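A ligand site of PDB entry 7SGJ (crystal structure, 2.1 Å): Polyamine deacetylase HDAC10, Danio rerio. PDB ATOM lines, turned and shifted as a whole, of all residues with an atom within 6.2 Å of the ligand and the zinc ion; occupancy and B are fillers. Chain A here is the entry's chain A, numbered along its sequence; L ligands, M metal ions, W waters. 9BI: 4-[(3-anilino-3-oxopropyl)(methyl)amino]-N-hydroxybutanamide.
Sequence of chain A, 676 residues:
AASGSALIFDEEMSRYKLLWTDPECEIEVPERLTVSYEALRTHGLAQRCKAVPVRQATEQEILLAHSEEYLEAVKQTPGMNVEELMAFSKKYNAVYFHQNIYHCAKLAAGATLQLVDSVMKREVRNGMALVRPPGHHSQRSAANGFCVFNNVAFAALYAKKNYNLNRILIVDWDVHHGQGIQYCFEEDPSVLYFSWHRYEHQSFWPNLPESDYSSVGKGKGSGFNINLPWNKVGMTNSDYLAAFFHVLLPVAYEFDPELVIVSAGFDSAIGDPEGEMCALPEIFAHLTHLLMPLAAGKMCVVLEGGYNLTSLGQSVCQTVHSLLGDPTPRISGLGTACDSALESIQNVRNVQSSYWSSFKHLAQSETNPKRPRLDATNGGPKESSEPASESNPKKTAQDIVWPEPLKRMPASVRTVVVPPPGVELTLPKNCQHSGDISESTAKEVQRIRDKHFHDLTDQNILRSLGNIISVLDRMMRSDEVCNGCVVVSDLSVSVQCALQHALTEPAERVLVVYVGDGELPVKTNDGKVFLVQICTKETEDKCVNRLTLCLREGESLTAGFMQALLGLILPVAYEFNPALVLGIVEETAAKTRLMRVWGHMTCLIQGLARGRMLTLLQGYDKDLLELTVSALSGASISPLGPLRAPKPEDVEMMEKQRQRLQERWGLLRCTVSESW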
ATOM      1  N   GLU A  24     -20.968  -2.362  12.578  1.00  0.00           N
ATOM      2  CA  GLU A  24     -21.084  -1.441  11.461  1.00  0.00           C
ATOM      3  C   GLU A  24     -20.087  -0.282  11.540  1.00  0.00           C
ATOM      4  O   GLU A  24     -19.999   0.484  10.586  1.00  0.00           O
ATOM      5  CB  GLU A  24     -22.522  -0.888  11.382  1.00  0.00           C
ATOM      6  CG  GLU A  24     -23.610  -1.940  11.115  1.00  0.00           C
ATOM      7  CD  GLU A  24     -23.187  -3.036  10.118  1.00  0.00           C
ATOM      8  OE1 GLU A  24     -23.381  -4.233  10.450  1.00  0.00           O
ATOM      9  OE2 GLU A  24     -22.674  -2.719   9.018  1.00  0.00           O
ATOM     10  N   CYS A  25     -19.334  -0.156  12.635  1.00  0.00           N
ATOM     11  CA  CYS A  25     -18.383   0.927  12.793  1.00  0.00           C
ATOM     12  C   CYS A  25     -16.947   0.468  13.055  1.00  0.00           C
ATOM     13  O   CYS A  25     -16.037   1.310  12.979  1.00  0.00           O
ATOM     14  CB  CYS A  25     -18.821   1.870  13.942  1.00  0.00           C
ATOM     15  SG  CYS A  25     -20.344   2.847  13.591  1.00  0.00           S
ATOM     16  N   ILE A  27     -14.609  -0.818  11.441  1.00  0.00           N
ATOM     17  CA  ILE A  27     -13.565  -0.620  10.437  1.00  0.00           C
ATOM     18  C   ILE A  27     -12.960   0.768  10.473  1.00  0.00           C
ATOM     19  O   ILE A  27     -11.916   0.997   9.834  1.00  0.00           O
ATOM     20  CB  ILE A  27     -14.130  -0.879   9.031  1.00  0.00           C
ATOM     21  CG1 ILE A  27     -15.398  -0.031   8.832  1.00  0.00           C
ATOM     22  CG2 ILE A  27     -14.408  -2.370   8.819  1.00  0.00           C
ATOM     23  CD1 ILE A  27     -15.824   0.128   7.398  1.00  0.00           C
ATOM     24  N   ASN A  93     -27.114   7.578  12.133  1.00  0.00           N
ATOM     25  CA  ASN A  93     -26.897   6.339  11.406  1.00  0.00           C
ATOM     26  C   ASN A  93     -25.394   6.118  11.170  1.00  0.00           C
ATOM     27  O   ASN A  93     -24.732   6.974  10.568  1.00  0.00           O
ATOM     28  CB  ASN A  93     -27.624   6.356  10.063  1.00  0.00           C
ATOM     29  CG  ASN A  93     -27.546   5.036   9.347  1.00  0.00           C
ATOM     30  OD1 ASN A  93     -26.892   4.906   8.313  1.00  0.00           O
ATOM     31  ND2 ASN A  93     -28.198   4.014   9.906  1.00  0.00           N
ATOM     32  N   ALA A  94     -24.888   4.961  11.606  1.00  0.00           N
ATOM     33  CA  ALA A  94     -23.531   4.480  11.313  1.00  0.00           C
ATOM     34  C   ALA A  94     -22.450   5.494  11.719  1.00  0.00           C
ATOM     35  O   ALA A  94     -21.606   5.899  10.916  1.00  0.00           O
ATOM     36  CB  ALA A  94     -23.413   4.094   9.839  1.00  0.00           C
ATOM     37  N   PRO A 134     -13.785  11.426   8.690  1.00  0.00           N
ATOM     38  CA  PRO A 134     -14.179  11.843   7.337  1.00  0.00           C
ATOM     39  C   PRO A 134     -15.396  12.774   7.379  1.00  0.00           C
ATOM     40  O   PRO A 134     -15.999  13.019   8.432  1.00  0.00           O
ATOM     41  CB  PRO A 134     -14.501  10.533   6.620  1.00  0.00           C
ATOM     42  CG  PRO A 134     -14.963   9.609   7.756  1.00  0.00           C
ATOM     43  CD  PRO A 134     -14.045   9.987   8.919  1.00  0.00           C
ATOM     44  N   HIS A 136     -17.871  13.322   4.164  1.00  0.00           N
ATOM     45  CA  HIS A 136     -18.776  13.547   3.029  1.00  0.00           C
ATOM     46  C   HIS A 136     -20.204  13.070   3.302  1.00  0.00           C
ATOM     47  O   HIS A 136     -21.121  13.532   2.604  1.00  0.00           O
ATOM     48  CB  HIS A 136     -18.210  12.921   1.718  1.00  0.00           C
ATOM     49  CG  HIS A 136     -18.154  11.425   1.681  1.00  0.00           C
ATOM     50  ND1 HIS A 136     -18.247  10.716   0.494  1.00  0.00           N
ATOM     51  CD2 HIS A 136     -17.948  10.496   2.656  1.00  0.00           C
ATOM     52  CE1 HIS A 136     -18.135   9.420   0.740  1.00  0.00           C
ATOM     53  NE2 HIS A 136     -17.943   9.259   2.049  1.00  0.00           N
ATOM     54  N   HIS A 137     -20.450  12.264   4.334  1.00  0.00           N
ATOM     55  CA  HIS A 137     -21.815  11.922   4.719  1.00  0.00           C
ATOM     56  C   HIS A 137     -22.451  12.911   5.669  1.00  0.00           C
ATOM     57  O   HIS A 137     -23.669  12.846   5.886  1.00  0.00           O
ATOM     58  CB  HIS A 137     -21.851  10.538   5.358  1.00  0.00           C
ATOM     59  CG  HIS A 137     -21.387   9.449   4.443  1.00  0.00           C
ATOM     60  ND1 HIS A 137     -21.900   9.301   3.167  1.00  0.00           N
ATOM     61  CD2 HIS A 137     -20.443   8.501   4.591  1.00  0.00           C
ATOM     62  CE1 HIS A 137     -21.273   8.294   2.573  1.00  0.00           C
ATOM     63  NE2 HIS A 137     -20.391   7.792   3.420  1.00  0.00           N
ATOM     64  N   GLY A 145     -22.463   8.082   8.920  1.00  0.00           N
ATOM     65  CA  GLY A 145     -21.421   7.335   8.208  1.00  0.00           C
ATOM     66  C   GLY A 145     -19.997   7.709   8.605  1.00  0.00           C
ATOM     67  O   GLY A 145     -19.191   8.048   7.738  1.00  0.00           O
ATOM     68  N   PHE A 146     -19.703   7.669   9.908  1.00  0.00           N
ATOM     69  CA  PHE A 146     -18.411   7.991  10.513  1.00  0.00           C
ATOM     70  C   PHE A 146     -18.058   9.477  10.418  1.00  0.00           C
ATOM     71  O   PHE A 146     -16.991   9.867  10.922  1.00  0.00           O
ATOM     72  CB  PHE A 146     -17.231   7.198   9.907  1.00  0.00           C
ATOM     73  CG  PHE A 146     -17.515   5.721   9.688  1.00  0.00           C
ATOM     74  CD1 PHE A 146     -18.374   5.025  10.535  1.00  0.00           C
ATOM     75  CD2 PHE A 146     -16.900   5.041   8.649  1.00  0.00           C
ATOM     76  CE1 PHE A 146     -18.626   3.685  10.326  1.00  0.00           C
ATOM     77  CE2 PHE A 146     -17.141   3.700   8.457  1.00  0.00           C
ATOM     78  CZ  PHE A 146     -18.013   3.024   9.302  1.00  0.00           C
ATOM     79  N   CYS A 147     -18.893  10.313   9.796  1.00  0.00           N
ATOM     80  CA  CYS A 147     -18.631  11.729   9.577  1.00  0.00           C
ATOM     81  C   CYS A 147     -19.379  12.590  10.590  1.00  0.00           C
ATOM     82  O   CYS A 147     -20.571  12.383  10.816  1.00  0.00           O
ATOM     83  CB  CYS A 147     -19.038  12.158   8.172  1.00  0.00           C
ATOM     84  SG  CYS A 147     -18.360  11.137   6.889  1.00  0.00           S
ATOM     85  N   ASP A 174     -14.562   8.293  -3.296  1.00  0.00           N
ATOM     86  CA  ASP A 174     -14.896   7.317  -2.259  1.00  0.00           C
ATOM     87  C   ASP A 174     -15.931   6.344  -2.823  1.00  0.00           C
ATOM     88  O   ASP A 174     -16.654   6.682  -3.773  1.00  0.00           O
ATOM     89  CB  ASP A 174     -15.452   8.049  -1.011  1.00  0.00           C
ATOM     90  CG  ASP A 174     -15.659   7.135   0.185  1.00  0.00           C
ATOM     91  OD1 ASP A 174     -14.832   7.155   1.119  1.00  0.00           O
ATOM     92  OD2 ASP A 174     -16.681   6.415   0.253  1.00  0.00           O
ATOM     93  N   VAL A 175     -15.992   5.137  -2.254  1.00  0.00           N
ATOM     94  CA  VAL A 175     -16.904   4.136  -2.811  1.00  0.00           C
ATOM     95  C   VAL A 175     -18.337   4.323  -2.342  1.00  0.00           C
ATOM     96  O   VAL A 175     -19.247   3.659  -2.855  1.00  0.00           O
ATOM     97  CB  VAL A 175     -16.417   2.705  -2.478  1.00  0.00           C
ATOM     98  CG1 VAL A 175     -16.922   2.244  -1.106  1.00  0.00           C
ATOM     99  CG2 VAL A 175     -16.856   1.737  -3.586  1.00  0.00           C
ATOM    100  N   HIS A 176     -18.573   5.206  -1.374  1.00  0.00           N
ATOM    101  CA  HIS A 176     -19.901   5.494  -0.864  1.00  0.00           C
ATOM    102  C   HIS A 176     -20.369   6.830  -1.417  1.00  0.00           C
ATOM    103  O   HIS A 176     -19.570   7.715  -1.745  1.00  0.00           O
ATOM    104  CB  HIS A 176     -19.915   5.539   0.661  1.00  0.00           C
ATOM    105  CG  HIS A 176     -19.558   4.248   1.325  1.00  0.00           C
ATOM    106  ND1 HIS A 176     -18.269   3.938   1.705  1.00  0.00           N
ATOM    107  CD2 HIS A 176     -20.322   3.196   1.703  1.00  0.00           C
ATOM    108  CE1 HIS A 176     -18.256   2.755   2.296  1.00  0.00           C
ATOM    109  NE2 HIS A 176     -19.487   2.285   2.297  1.00  0.00           N
ATOM    110  N   TRP A 205     -25.819   0.604   1.393  1.00  0.00           N
ATOM    111  CA  TRP A 205     -25.809   1.778   2.260  1.00  0.00           C
ATOM    112  C   TRP A 205     -25.236   2.987   1.509  1.00  0.00           C
ATOM    113  O   TRP A 205     -24.246   2.858   0.787  1.00  0.00           O
ATOM    114  CB  TRP A 205     -24.983   1.469   3.523  1.00  0.00           C
ATOM    115  CG  TRP A 205     -25.118   2.514   4.577  1.00  0.00           C
ATOM    116  CD1 TRP A 205     -26.018   2.520   5.624  1.00  0.00           C
ATOM    117  CD2 TRP A 205     -24.392   3.740   4.662  1.00  0.00           C
ATOM    118  NE1 TRP A 205     -25.872   3.682   6.350  1.00  0.00           N
ATOM    119  CE2 TRP A 205     -24.897   4.456   5.772  1.00  0.00           C
ATOM    120  CE3 TRP A 205     -23.373   4.310   3.888  1.00  0.00           C
ATOM    121  CZ2 TRP A 205     -24.398   5.707   6.153  1.00  0.00           C
ATOM    122  CZ3 TRP A 205     -22.863   5.563   4.261  1.00  0.00           C
ATOM    123  CH2 TRP A 205     -23.383   6.246   5.393  1.00  0.00           C
ATOM    124  N   ASN A 207     -28.474   3.580   0.940  1.00  0.00           N
ATOM    125  CA  ASN A 207     -29.791   3.129   0.469  1.00  0.00           C
ATOM    126  C   ASN A 207     -30.701   4.291   0.073  1.00  0.00           C
ATOM    127  O   ASN A 207     -31.859   4.331   0.477  1.00  0.00           O
ATOM    128  CB  ASN A 207     -30.495   2.261   1.539  1.00  0.00           C
ATOM    129  CG  ASN A 207     -29.604   1.185   2.106  1.00  0.00           C
ATOM    130  OD1 ASN A 207     -29.065   1.318   3.211  1.00  0.00           O
ATOM    131  ND2 ASN A 207     -29.466   0.085   1.371  1.00  0.00           N
ATOM    132  N   GLY A 265     -11.806   8.954  -0.926  1.00  0.00           N
ATOM    133  CA  GLY A 265     -11.937   7.716  -0.182  1.00  0.00           C
ATOM    134  C   GLY A 265     -11.370   6.590  -1.026  1.00  0.00           C
ATOM    135  O   GLY A 265     -11.659   6.490  -2.228  1.00  0.00           O
ATOM    136  N   ASP A 267     -11.708   3.403  -0.176  1.00  0.00           N
ATOM    137  CA  ASP A 267     -12.490   2.191  -0.106  1.00  0.00           C
ATOM    138  C   ASP A 267     -13.029   1.789  -1.479  1.00  0.00           C
ATOM    139  O   ASP A 267     -13.711   0.772  -1.571  1.00  0.00           O
ATOM    140  CB  ASP A 267     -13.637   2.321   0.908  1.00  0.00           C
ATOM    141  CG  ASP A 267     -14.440   3.598   0.763  1.00  0.00           C
ATOM    142  OD1 ASP A 267     -14.343   4.302  -0.264  1.00  0.00           O
ATOM    143  OD2 ASP A 267     -15.203   3.866   1.712  1.00  0.00           O
ATOM    144  N   GLU A 274     -15.495  -2.768   2.371  1.00  0.00           N
ATOM    145  CA  GLU A 274     -16.722  -2.034   2.122  1.00  0.00           C
ATOM    146  C   GLU A 274     -17.067  -1.963   0.635  1.00  0.00           C
ATOM    147  O   GLU A 274     -18.219  -2.170   0.244  1.00  0.00           O
ATOM    148  CB  GLU A 274     -16.635  -0.616   2.696  1.00  0.00           C
ATOM    149  CG  GLU A 274     -16.994  -0.542   4.143  1.00  0.00           C
ATOM    150  CD  GLU A 274     -18.463  -0.839   4.384  1.00  0.00           C
ATOM    151  OE1 GLU A 274     -19.324  -0.142   3.784  1.00  0.00           O
ATOM    152  OE2 GLU A 274     -18.747  -1.763   5.174  1.00  0.00           O
ATOM    153  N   GLU A 304     -11.202  10.730   2.771  1.00  0.00           N
ATOM    154  CA  GLU A 304     -12.493  10.270   3.293  1.00  0.00           C
ATOM    155  C   GLU A 304     -12.327   8.874   3.893  1.00  0.00           C
ATOM    156  O   GLU A 304     -11.730   8.723   4.962  1.00  0.00           O
ATOM    157  CB  GLU A 304     -13.563  10.294   2.207  1.00  0.00           C
ATOM    158  CG  GLU A 304     -13.815  11.690   1.621  1.00  0.00           C
ATOM    159  CD  GLU A 304     -14.690  12.584   2.518  1.00  0.00           C
ATOM    160  OE1 GLU A 304     -15.172  12.124   3.573  1.00  0.00           O
ATOM    161  OE2 GLU A 304     -14.913  13.767   2.134  1.00  0.00           O
ATOM    162  N   GLY A 305     -12.829   7.841   3.215  1.00  0.00           N
ATOM    163  CA  GLY A 305     -12.765   6.460   3.692  1.00  0.00           C
ATOM    164  C   GLY A 305     -11.596   5.677   3.120  1.00  0.00           C
ATOM    165  O   GLY A 305     -10.677   6.224   2.494  1.00  0.00           O
ATOM    166  N   GLY A 306     -11.639   4.354   3.331  1.00  0.00           N
ATOM    167  CA  GLY A 306     -10.586   3.427   2.899  1.00  0.00           C
ATOM    168  C   GLY A 306     -10.092   2.581   4.064  1.00  0.00           C
ATOM    169  O   GLY A 306      -9.450   3.115   4.955  1.00  0.00           O
ATOM    170  N   TYR A 307     -10.366   1.267   4.060  1.00  0.00           N
ATOM    171  CA  TYR A 307     -10.325   0.471   5.291  1.00  0.00           C
ATOM    172  C   TYR A 307      -9.425  -0.758   5.253  1.00  0.00           C
ATOM    173  O   TYR A 307      -9.187  -1.338   6.313  1.00  0.00           O
ATOM    174  CB  TYR A 307     -11.742   0.039   5.684  1.00  0.00           C
ATOM    175  CG  TYR A 307     -12.647   1.250   5.761  1.00  0.00           C
ATOM    176  CD1 TYR A 307     -12.567   2.112   6.842  1.00  0.00           C
ATOM    177  CD2 TYR A 307     -13.509   1.566   4.725  1.00  0.00           C
ATOM    178  CE1 TYR A 307     -13.345   3.246   6.907  1.00  0.00           C
ATOM    179  CE2 TYR A 307     -14.310   2.686   4.781  1.00  0.00           C
ATOM    180  CZ  TYR A 307     -14.216   3.519   5.875  1.00  0.00           C
ATOM    181  OH  TYR A 307     -14.988   4.642   5.923  1.00  0.00           O
HETATM  182  C10 9BI L   1     -22.307   1.743   7.353  1.00  0.00           C
HETATM  183  C15 9BI L   1     -26.601  -0.745   8.275  1.00  0.00           C
HETATM  184  C17 9BI L   1     -28.252  -2.068   9.436  1.00  0.00           C
HETATM  185  C20 9BI L   1     -27.347   0.404   8.543  1.00  0.00           C
HETATM  186  C01 9BI L   1     -20.120   0.914   6.942  1.00  0.00           C
HETATM  187  C03 9BI L   1     -20.625   3.238   6.580  1.00  0.00           C
HETATM  188  C04 9BI L   1     -19.516   3.513   5.558  1.00  0.00           C
HETATM  189  C05 9BI L   1     -19.098   4.994   5.551  1.00  0.00           C
HETATM  190  C06 9BI L   1     -17.959   5.356   4.599  1.00  0.00           C
HETATM  191  C11 9BI L   1     -22.947   0.346   7.242  1.00  0.00           C
HETATM  192  C12 9BI L   1     -24.273   0.221   8.011  1.00  0.00           C
HETATM  193  C16 9BI L   1     -27.055  -1.980   8.736  1.00  0.00           C
HETATM  194  C18 9BI L   1     -28.998  -0.918   9.703  1.00  0.00           C
HETATM  195  C19 9BI L   1     -28.549   0.314   9.259  1.00  0.00           C
HETATM  196  N02 9BI L   1     -21.127   1.868   6.505  1.00  0.00           N
HETATM  197  N08 9BI L   1     -18.109   6.523   3.761  1.00  0.00           N
HETATM  198  N14 9BI L   1     -25.348  -0.649   7.534  1.00  0.00           N
HETATM  199  O07 9BI L   1     -16.970   4.714   4.520  1.00  0.00           O
HETATM  200  O09 9BI L   1     -17.136   6.968   2.863  1.00  0.00           O
HETATM  201  O13 9BI L   1     -24.427   0.841   9.027  1.00  0.00           O
HETATM  202 ZN    ZN M   1     -16.585   5.312   1.835  1.00  0.00          ZN
HETATM  203  O   HOH W   1     -21.863   0.464   4.142  1.00  0.00           O
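The side-chain carboxylate of Asp 267 lies within hydrogen-bond range of the backbone NH of Val 175 (2.7 Å). NE2 of His 137 is in hydrogen-bond range of NE2 of His 136, at 3.2 Å. The backbone NH (N) of His 136 sits at hydrogen-bond distance from the side-chain carboxylate (OE1) of Glu 304, 3.0 Å away. SG of Cys 147 sits at hydrogen-bond distance from N of His 136, 3.5 Å away. N of His 137 sits at hydrogen-bond distance from SG of Cys 147, 3.5 Å away. The indole nitrogen (NE1) of Trp 205 lies within hydrogen-bond range of the side-chain amide oxygen (OD1) of Asn 93 (2.5 Å). The backbone NH (N) of Gly 145 sits at hydrogen-bond distance from the backbone carbonyl oxygen (O) of Asn 93, 3.0 Å away. O of Gly 145 sits at hydrogen-bond distance from SG of Cys 147, at 3.3 Å.
The zinc ion is bound by OD2 of Asp 174 (1.9 Å), OD2 of Asp 267 (2.0 Å), O09 of the ligand (2.0 Å) and ND1 of His 176 (2.2 Å). The zinc ion has four donor atoms within binding distance. Slightly farther from the zinc ion lies OD1 of Asp 174 (2.6 Å). Slightly farther from the zinc ion lies an oxygen (O07) of the ligand (2.8 Å).
An oxygen (O07) of the ligand lies within hydrogen-bond range of the side-chain hydroxyl of Tyr 307 (2.4 Å). A nitrogen (N08) of the ligand lies within hydrogen-bond range of a ring nitrogen (NE2) of His 136, 3.2 Å away. A ring nitrogen (NE2) of His 137 is in hydrogen-bond range of a nitrogen (N08) of the ligand (2.6 Å). OE1 of Glu 274 lies within salt-bridge range of N02 of the ligand, 3.8 Å away.
CB of Glu 24 touches O13 of the ligand, 3.5 Å away. Asn 93 touches the ligand (ND2 to C19, 3.8 Å). CB of Ala 94 touches O13 of the ligand (3.5 Å). Gly 145 touches the ligand (O to C05, 3.8 Å). Phe 146 touches the ligand. CD1 of Trp 205 touches C12 of the ligand, at 3.7 Å. Hydrophobic or aromatic side chains that line the ligand: Ala 94, His 136, His 137, Phe 146, His 176, Trp 205 and Tyr 307. Of the 23 residues printed, 13 come within 4 Å of the ligand.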
